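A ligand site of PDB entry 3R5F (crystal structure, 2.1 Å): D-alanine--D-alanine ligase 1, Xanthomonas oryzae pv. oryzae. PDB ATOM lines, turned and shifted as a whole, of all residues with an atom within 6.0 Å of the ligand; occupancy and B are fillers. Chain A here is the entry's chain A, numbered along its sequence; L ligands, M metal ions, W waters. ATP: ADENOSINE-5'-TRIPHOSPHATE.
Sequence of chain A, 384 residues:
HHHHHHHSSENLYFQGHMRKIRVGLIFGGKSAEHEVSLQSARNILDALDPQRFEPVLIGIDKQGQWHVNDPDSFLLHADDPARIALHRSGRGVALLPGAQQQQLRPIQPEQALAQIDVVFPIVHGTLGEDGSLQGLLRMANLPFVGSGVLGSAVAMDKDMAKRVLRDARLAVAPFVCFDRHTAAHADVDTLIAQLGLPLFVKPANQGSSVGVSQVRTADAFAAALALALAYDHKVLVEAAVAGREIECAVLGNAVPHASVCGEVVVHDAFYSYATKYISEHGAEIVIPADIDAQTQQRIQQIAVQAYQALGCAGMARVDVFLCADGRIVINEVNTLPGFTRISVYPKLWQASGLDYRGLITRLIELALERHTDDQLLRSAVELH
The side-chain carboxylate of Glu 245 is in hydrogen-bond range of an oxygen (O2') of the ligand (2.5 Å).
The side-chain hydroxyl (OG) of Ser 209 is in hydrogen-bond range of an oxygen (O2G) of the ligand, at 2.6 Å.
The side-chain carboxylate of Glu 332 sits close to an oxygen (O1B) of the ligand, 2.6 Å away.
N of Val 241 lies within hydrogen-bond range of N1 of the ligand, at 2.7 Å.
The backbone carbonyl oxygen (O) of Ala 239 sits at hydrogen-bond distance from a nitrogen (N6) of the ligand (2.8 Å).
The side-chain amino group (NZ) of Lys 202 is in salt-bridge range of an oxygen (O2A) of the ligand (2.9 Å).
A nitrogen (N6) of the ligand lies within hydrogen-bond range of the side-chain carboxylate (OE1) of Glu 238, 2.9 Å away.
An oxygen (O2A) of the ligand lies within salt-bridge range of the side-chain amino group (NZ) of Lys 158 (3.2 Å).
The backbone carbonyl oxygen of Glu 332 is in hydrogen-bond range of the backbone NH of Asp 319 (2.8 Å).
The guanidinium group (NH2) of Arg 317 is in salt-bridge range of the side-chain carboxylate (OE1) of Glu 332, 3.6 Å away.
OE1 of Gln 206 lies close to OE1 of Glu 332 (3.5 Å).
The side-chain amide nitrogen of Asn 334 is in hydrogen-bond range of the side-chain carboxylate of Glu 332.
The side-chain amino group (NZ) of Lys 202 lies within salt-bridge range of the side-chain carboxylate (OE1) of Glu 238 (3.0 Å).
The side-chain amino group of Lys 202 sits at hydrogen-bond distance from the side-chain amide oxygen of Asn 331.
The backbone carbonyl oxygen of Phe 200 sits at hydrogen-bond distance from the backbone NH of Glu 238 (2.7 Å).
The backbone carbonyl oxygen (O) of Asp 319 is in hydrogen-bond range of the backbone NH (N) of Asn 331 (2.9 Å).
An oxygen (O2B) of the ligand lies close to the backbone carbonyl oxygen of Ser 208 (3.5 Å).
Residues that only touch the ligand: Phe 200 (3.4 Å), Ala 240 (3.4 Å), Phe 321 (3.6 Å) and Asn 331 (3.5 Å).
Hydrophobic or aromatic side chains within 4 Å of the ligand: Phe 200, Val 241 and Phe 321.
Of the 21 residues printed, 13 come within 4 Å of the ligand.
Water W1 lies within hydrogen-bond range of O1B of the ligand, OE1 of Glu 332 and O of Gln 206.
Water W3 bridges the side-chain carboxylate (OD2) of Asp 319 (2.7 Å) and an oxygen (O3G) of the ligand (3.2 Å).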
ATOM      1  N   LYS A 158     -20.279   6.278 -16.782  1.00  0.00           N
ATOM      2  CA  LYS A 158     -20.723   6.451 -15.434  1.00  0.00           C
ATOM      3  C   LYS A 158     -19.635   6.140 -14.420  1.00  0.00           C
ATOM      4  O   LYS A 158     -19.667   6.676 -13.353  1.00  0.00           O
ATOM      5  CB  LYS A 158     -21.929   5.568 -15.162  1.00  0.00           C
ATOM      6  CG  LYS A 158     -23.194   5.935 -15.899  1.00  0.00           C
ATOM      7  CD  LYS A 158     -24.220   4.699 -15.808  1.00  0.00           C
ATOM      8  CE  LYS A 158     -25.653   5.156 -15.513  1.00  0.00           C
ATOM      9  NZ  LYS A 158     -25.756   5.399 -14.023  1.00  0.00           N
ATOM     10  N   ALA A 173     -23.329   6.899  -5.286  1.00  0.00           N
ATOM     11  CA  ALA A 173     -23.474   5.535  -4.654  1.00  0.00           C
ATOM     12  C   ALA A 173     -22.141   4.839  -4.560  1.00  0.00           C
ATOM     13  O   ALA A 173     -21.399   4.728  -5.551  1.00  0.00           O
ATOM     14  CB  ALA A 173     -24.377   4.712  -5.469  1.00  0.00           C
ATOM     15  N   PHE A 200     -27.104  -2.831  -7.485  1.00  0.00           N
ATOM     16  CA  PHE A 200     -27.525  -2.383  -8.802  1.00  0.00           C
ATOM     17  C   PHE A 200     -26.361  -2.610  -9.748  1.00  0.00           C
ATOM     18  O   PHE A 200     -25.235  -2.144  -9.538  1.00  0.00           O
ATOM     19  CB  PHE A 200     -28.042  -0.932  -8.767  1.00  0.00           C
ATOM     20  CG  PHE A 200     -29.405  -0.812  -8.081  1.00  0.00           C
ATOM     21  CD1 PHE A 200     -29.491  -0.719  -6.661  1.00  0.00           C
ATOM     22  CD2 PHE A 200     -30.580  -0.886  -8.840  1.00  0.00           C
ATOM     23  CE1 PHE A 200     -30.720  -0.632  -6.014  1.00  0.00           C
ATOM     24  CE2 PHE A 200     -31.872  -0.831  -8.213  1.00  0.00           C
ATOM     25  CZ  PHE A 200     -31.941  -0.679  -6.806  1.00  0.00           C
ATOM     26  N   LYS A 202     -24.851  -2.356 -13.565  1.00  0.00           N
ATOM     27  CA  LYS A 202     -25.074  -1.570 -14.799  1.00  0.00           C
ATOM     28  C   LYS A 202     -23.861  -1.372 -15.698  1.00  0.00           C
ATOM     29  O   LYS A 202     -22.708  -1.263 -15.214  1.00  0.00           O
ATOM     30  CB  LYS A 202     -25.894  -0.302 -14.496  1.00  0.00           C
ATOM     31  CG  LYS A 202     -25.395   0.694 -13.444  1.00  0.00           C
ATOM     32  CD  LYS A 202     -26.576   1.092 -12.441  1.00  0.00           C
ATOM     33  CE  LYS A 202     -26.363   2.514 -11.911  1.00  0.00           C
ATOM     34  NZ  LYS A 202     -27.458   3.308 -11.176  1.00  0.00           N
ATOM     35  N   GLN A 206     -23.710   5.014 -20.411  1.00  0.00           N
ATOM     36  CA  GLN A 206     -25.067   5.412 -20.097  1.00  0.00           C
ATOM     37  C   GLN A 206     -25.902   5.678 -21.335  1.00  0.00           C
ATOM     38  O   GLN A 206     -26.982   6.170 -21.268  1.00  0.00           O
ATOM     39  CB  GLN A 206     -25.095   6.555 -19.092  1.00  0.00           C
ATOM     40  CG  GLN A 206     -25.126   7.903 -19.654  1.00  0.00           C
ATOM     41  CD  GLN A 206     -25.298   8.948 -18.589  1.00  0.00           C
ATOM     42  OE1 GLN A 206     -26.012   9.877 -18.777  1.00  0.00           O
ATOM     43  NE2 GLN A 206     -24.654   8.768 -17.464  1.00  0.00           N
ATOM     44  N   SER A 208     -27.433   3.578 -23.163  1.00  0.00           N
ATOM     45  CA  SER A 208     -28.682   2.839 -23.097  1.00  0.00           C
ATOM     46  C   SER A 208     -29.077   2.690 -21.620  1.00  0.00           C
ATOM     47  O   SER A 208     -28.217   2.720 -20.740  1.00  0.00           O
ATOM     48  CB  SER A 208     -28.443   1.444 -23.700  1.00  0.00           C
ATOM     49  OG  SER A 208     -27.101   0.990 -23.434  1.00  0.00           O
ATOM     50  N   SER A 209     -30.375   2.490 -21.346  1.00  0.00           N
ATOM     51  CA  SER A 209     -30.847   2.104 -20.015  1.00  0.00           C
ATOM     52  C   SER A 209     -30.908   0.567 -19.931  1.00  0.00           C
ATOM     53  O   SER A 209     -31.288  -0.044 -18.945  1.00  0.00           O
ATOM     54  CB  SER A 209     -32.197   2.723 -19.702  1.00  0.00           C
ATOM     55  OG  SER A 209     -32.178   4.097 -20.069  1.00  0.00           O
ATOM     56  N   VAL A 210     -30.505  -0.058 -21.015  1.00  0.00           N
ATOM     57  CA  VAL A 210     -30.489  -1.494 -21.124  1.00  0.00           C
ATOM     58  C   VAL A 210     -29.405  -1.952 -20.219  1.00  0.00           C
ATOM     59  O   VAL A 210     -28.562  -1.170 -19.863  1.00  0.00           O
ATOM     60  CB  VAL A 210     -30.125  -1.889 -22.524  1.00  0.00           C
ATOM     61  CG1 VAL A 210     -30.668  -0.892 -23.476  1.00  0.00           C
ATOM     62  CG2 VAL A 210     -28.678  -1.983 -22.647  1.00  0.00           C
ATOM     63  N   VAL A 212     -29.554  -2.864 -16.964  1.00  0.00           N
ATOM     64  CA  VAL A 212     -29.617  -2.553 -15.533  1.00  0.00           C
ATOM     65  C   VAL A 212     -30.448  -3.482 -14.688  1.00  0.00           C
ATOM     66  O   VAL A 212     -31.644  -3.398 -14.693  1.00  0.00           O
ATOM     67  CB  VAL A 212     -30.230  -1.182 -15.294  1.00  0.00           C
ATOM     68  CG1 VAL A 212     -30.003  -0.768 -13.904  1.00  0.00           C
ATOM     69  CG2 VAL A 212     -29.647  -0.233 -16.205  1.00  0.00           C
ATOM     70  N   GLU A 238     -23.319  -1.253  -7.895  1.00  0.00           N
ATOM     71  CA  GLU A 238     -23.498  -0.215  -6.872  1.00  0.00           C
ATOM     72  C   GLU A 238     -24.297  -0.671  -5.685  1.00  0.00           C
ATOM     73  O   GLU A 238     -25.230  -1.472  -5.848  1.00  0.00           O
ATOM     74  CB  GLU A 238     -24.338   0.905  -7.437  1.00  0.00           C
ATOM     75  CG  GLU A 238     -23.771   1.545  -8.610  1.00  0.00           C
ATOM     76  CD  GLU A 238     -24.540   2.822  -9.018  1.00  0.00           C
ATOM     77  OE1 GLU A 238     -25.733   3.013  -8.729  1.00  0.00           O
ATOM     78  OE2 GLU A 238     -23.888   3.671  -9.682  1.00  0.00           O
ATOM     79  N   ALA A 239     -24.027  -0.080  -4.528  1.00  0.00           N
ATOM     80  CA  ALA A 239     -24.894  -0.227  -3.324  1.00  0.00           C
ATOM     81  C   ALA A 239     -26.253   0.461  -3.608  1.00  0.00           C
ATOM     82  O   ALA A 239     -26.327   1.402  -4.397  1.00  0.00           O
ATOM     83  CB  ALA A 239     -24.201   0.429  -2.126  1.00  0.00           C
ATOM     84  N   ALA A 240     -27.330  -0.010  -2.987  1.00  0.00           N
ATOM     85  CA  ALA A 240     -28.628   0.636  -3.140  1.00  0.00           C
ATOM     86  C   ALA A 240     -28.552   1.961  -2.385  1.00  0.00           C
ATOM     87  O   ALA A 240     -27.928   2.056  -1.283  1.00  0.00           O
ATOM     88  CB  ALA A 240     -29.748  -0.248  -2.624  1.00  0.00           C
ATOM     89  N   VAL A 241     -29.118   2.994  -2.986  1.00  0.00           N
ATOM     90  CA  VAL A 241     -29.317   4.217  -2.229  1.00  0.00           C
ATOM     91  C   VAL A 241     -30.806   4.316  -1.890  1.00  0.00           C
ATOM     92  O   VAL A 241     -31.653   4.477  -2.802  1.00  0.00           O
ATOM     93  CB  VAL A 241     -28.822   5.480  -2.990  1.00  0.00           C
ATOM     94  CG1 VAL A 241     -28.868   6.690  -2.086  1.00  0.00           C
ATOM     95  CG2 VAL A 241     -27.369   5.232  -3.498  1.00  0.00           C
ATOM     96  N   ALA A 242     -31.126   4.228  -0.593  1.00  0.00           N
ATOM     97  CA  ALA A 242     -32.480   4.456  -0.089  1.00  0.00           C
ATOM     98  C   ALA A 242     -32.791   5.954  -0.006  1.00  0.00           C
ATOM     99  O   ALA A 242     -32.191   6.699   0.805  1.00  0.00           O
ATOM    100  CB  ALA A 242     -32.622   3.851   1.310  1.00  0.00           C
ATOM    101  N   GLU A 245     -36.263  10.182  -5.394  1.00  0.00           N
ATOM    102  CA  GLU A 245     -35.592  10.502  -6.619  1.00  0.00           C
ATOM    103  C   GLU A 245     -35.920  11.876  -7.072  1.00  0.00           C
ATOM    104  O   GLU A 245     -37.027  12.167  -7.388  1.00  0.00           O
ATOM    105  CB  GLU A 245     -36.001   9.508  -7.692  1.00  0.00           C
ATOM    106  CG  GLU A 245     -35.476   8.174  -7.455  1.00  0.00           C
ATOM    107  CD  GLU A 245     -35.547   7.291  -8.635  1.00  0.00           C
ATOM    108  OE1 GLU A 245     -35.366   6.107  -8.475  1.00  0.00           O
ATOM    109  OE2 GLU A 245     -35.790   7.781  -9.741  1.00  0.00           O
ATOM    110  N   ARG A 317     -29.430  17.204 -17.425  1.00  0.00           N
ATOM    111  CA  ARG A 317     -30.361  16.867 -16.324  1.00  0.00           C
ATOM    112  C   ARG A 317     -29.529  16.126 -15.259  1.00  0.00           C
ATOM    113  O   ARG A 317     -28.799  15.172 -15.635  1.00  0.00           O
ATOM    114  CB  ARG A 317     -31.549  16.039 -16.863  1.00  0.00           C
ATOM    115  CG  ARG A 317     -32.581  15.652 -15.769  1.00  0.00           C
ATOM    116  CD  ARG A 317     -33.597  14.563 -16.253  1.00  0.00           C
ATOM    117  NE  ARG A 317     -32.951  13.274 -16.177  1.00  0.00           N
ATOM    118  CZ  ARG A 317     -32.586  12.532 -17.247  1.00  0.00           C
ATOM    119  NH1 ARG A 317     -32.907  12.876 -18.515  1.00  0.00           N
ATOM    120  NH2 ARG A 317     -31.922  11.416 -17.041  1.00  0.00           N
ATOM    121  N   ASP A 319     -29.758  13.797 -11.888  1.00  0.00           N
ATOM    122  CA  ASP A 319     -30.756  12.929 -11.126  1.00  0.00           C
ATOM    123  C   ASP A 319     -30.044  12.583  -9.851  1.00  0.00           C
ATOM    124  O   ASP A 319     -28.883  12.103  -9.908  1.00  0.00           O
ATOM    125  CB  ASP A 319     -31.033  11.655 -11.901  1.00  0.00           C
ATOM    126  CG  ASP A 319     -31.585  11.899 -13.281  1.00  0.00           C
ATOM    127  OD1 ASP A 319     -32.079  13.009 -13.552  1.00  0.00           O
ATOM    128  OD2 ASP A 319     -31.578  10.971 -14.110  1.00  0.00           O
ATOM    129  N   PHE A 321     -30.541  11.225  -5.554  1.00  0.00           N
ATOM    130  CA  PHE A 321     -31.331  10.581  -4.467  1.00  0.00           C
ATOM    131  C   PHE A 321     -31.289  11.509  -3.308  1.00  0.00           C
ATOM    132  O   PHE A 321     -30.231  12.069  -3.002  1.00  0.00           O
ATOM    133  CB  PHE A 321     -30.708   9.257  -4.001  1.00  0.00           C
ATOM    134  CG  PHE A 321     -30.696   8.188  -5.056  1.00  0.00           C
ATOM    135  CD1 PHE A 321     -31.846   7.551  -5.438  1.00  0.00           C
ATOM    136  CD2 PHE A 321     -29.484   7.786  -5.620  1.00  0.00           C
ATOM    137  CE1 PHE A 321     -31.806   6.526  -6.437  1.00  0.00           C
ATOM    138  CE2 PHE A 321     -29.437   6.760  -6.577  1.00  0.00           C
ATOM    139  CZ  PHE A 321     -30.616   6.148  -7.017  1.00  0.00           C
ATOM    140  N   ASN A 331     -26.996  10.268  -8.679  1.00  0.00           N
ATOM    141  CA  ASN A 331     -27.157   9.034  -9.472  1.00  0.00           C
ATOM    142  C   ASN A 331     -26.565   9.189 -10.859  1.00  0.00           C
ATOM    143  O   ASN A 331     -25.717   8.387 -11.302  1.00  0.00           O
ATOM    144  CB  ASN A 331     -28.639   8.731  -9.584  1.00  0.00           C
ATOM    145  CG  ASN A 331     -28.901   7.474 -10.325  1.00  0.00           C
ATOM    146  OD1 ASN A 331     -28.140   6.494 -10.212  1.00  0.00           O
ATOM    147  ND2 ASN A 331     -29.946   7.480 -11.129  1.00  0.00           N
ATOM    148  N   GLU A 332     -27.004  10.234 -11.567  1.00  0.00           N
ATOM    149  CA  GLU A 332     -26.635  10.483 -12.955  1.00  0.00           C
ATOM    150  C   GLU A 332     -26.556  11.943 -13.355  1.00  0.00           C
ATOM    151  O   GLU A 332     -27.376  12.692 -12.927  1.00  0.00           O
ATOM    152  CB  GLU A 332     -27.721   9.851 -13.807  1.00  0.00           C
ATOM    153  CG  GLU A 332     -27.424   9.757 -15.263  1.00  0.00           C
ATOM    154  CD  GLU A 332     -28.436   8.923 -16.032  1.00  0.00           C
ATOM    155  OE1 GLU A 332     -28.964   9.396 -17.021  1.00  0.00           O
ATOM    156  OE2 GLU A 332     -28.690   7.805 -15.667  1.00  0.00           O
ATOM    157  N   ASN A 334     -26.883  13.696 -16.959  1.00  0.00           N
ATOM    158  CA  ASN A 334     -27.222  13.343 -18.319  1.00  0.00           C
ATOM    159  C   ASN A 334     -27.055  14.517 -19.262  1.00  0.00           C
ATOM    160  O   ASN A 334     -27.722  15.485 -19.111  1.00  0.00           O
ATOM    161  CB  ASN A 334     -28.645  12.900 -18.385  1.00  0.00           C
ATOM    162  CG  ASN A 334     -28.897  11.962 -19.495  1.00  0.00           C
ATOM    163  OD1 ASN A 334     -28.757  12.284 -20.668  1.00  0.00           O
ATOM    164  ND2 ASN A 334     -29.252  10.754 -19.126  1.00  0.00           N
HETATM  165  PG  ATP L   1     -33.005   5.528 -16.781  1.00  0.00           P
HETATM  166  O1G ATP L   1     -34.338   5.046 -16.218  1.00  0.00           O
HETATM  167  O2G ATP L   1     -33.077   5.737 -18.285  1.00  0.00           O
HETATM  168  O3G ATP L   1     -32.291   6.635 -16.009  1.00  0.00           O
HETATM  169  PB  ATP L   1     -30.466   4.397 -16.763  1.00  0.00           P
HETATM  170  O1B ATP L   1     -30.042   5.852 -16.747  1.00  0.00           O
HETATM  171  O2B ATP L   1     -29.898   3.513 -17.833  1.00  0.00           O
HETATM  172  O3B ATP L   1     -32.051   4.252 -16.597  1.00  0.00           O
HETATM  173  PA  ATP L   1     -30.222   4.378 -13.903  1.00  0.00           P
HETATM  174  O1A ATP L   1     -31.119   5.596 -13.849  1.00  0.00           O
HETATM  175  O2A ATP L   1     -28.783   4.449 -13.447  1.00  0.00           O
HETATM  176  O3A ATP L   1     -30.063   3.696 -15.367  1.00  0.00           O
HETATM  177  O5' ATP L   1     -31.125   3.287 -13.092  1.00  0.00           O
HETATM  178  C5' ATP L   1     -32.532   3.171 -13.291  1.00  0.00           C
HETATM  179  C4' ATP L   1     -33.327   3.303 -11.994  1.00  0.00           C
HETATM  180  O4' ATP L   1     -32.991   2.230 -11.114  1.00  0.00           O
HETATM  181  C3' ATP L   1     -33.069   4.575 -11.158  1.00  0.00           C
HETATM  182  O3' ATP L   1     -33.966   5.648 -11.444  1.00  0.00           O
HETATM  183  C2' ATP L   1     -33.430   4.115  -9.771  1.00  0.00           C
HETATM  184  O2' ATP L   1     -34.863   3.988  -9.693  1.00  0.00           O
HETATM  185  C1' ATP L   1     -32.944   2.695  -9.756  1.00  0.00           C
HETATM  186  N9  ATP L   1     -31.539   2.677  -9.285  1.00  0.00           N
HETATM  187  C8  ATP L   1     -30.449   2.651 -10.056  1.00  0.00           C
HETATM  188  N7  ATP L   1     -29.340   2.589  -9.267  1.00  0.00           N
HETATM  189  C5  ATP L   1     -29.715   2.628  -7.989  1.00  0.00           C
HETATM  190  C6  ATP L   1     -29.026   2.614  -6.653  1.00  0.00           C
HETATM  191  N6  ATP L   1     -27.651   2.557  -6.546  1.00  0.00           N
HETATM  192  N1  ATP L   1     -29.853   2.659  -5.572  1.00  0.00           N
HETATM  193  C2  ATP L   1     -31.201   2.712  -5.648  1.00  0.00           C
HETATM  194  N3  ATP L   1     -31.874   2.737  -6.813  1.00  0.00           N
HETATM  195  C4  ATP L   1     -31.187   2.690  -7.993  1.00  0.00           C
HETATM  196 MG    MG M   1     -31.232   8.361 -13.954  1.00  0.00          MG
HETATM  197  O   HOH W   1     -29.491   7.009 -19.012  1.00  0.00           O
HETATM  198  O   HOH W   2     -34.260   6.451 -14.151  1.00  0.00           O
HETATM  199  O   HOH W   3     -33.582   9.282 -14.642  1.00  0.00           O
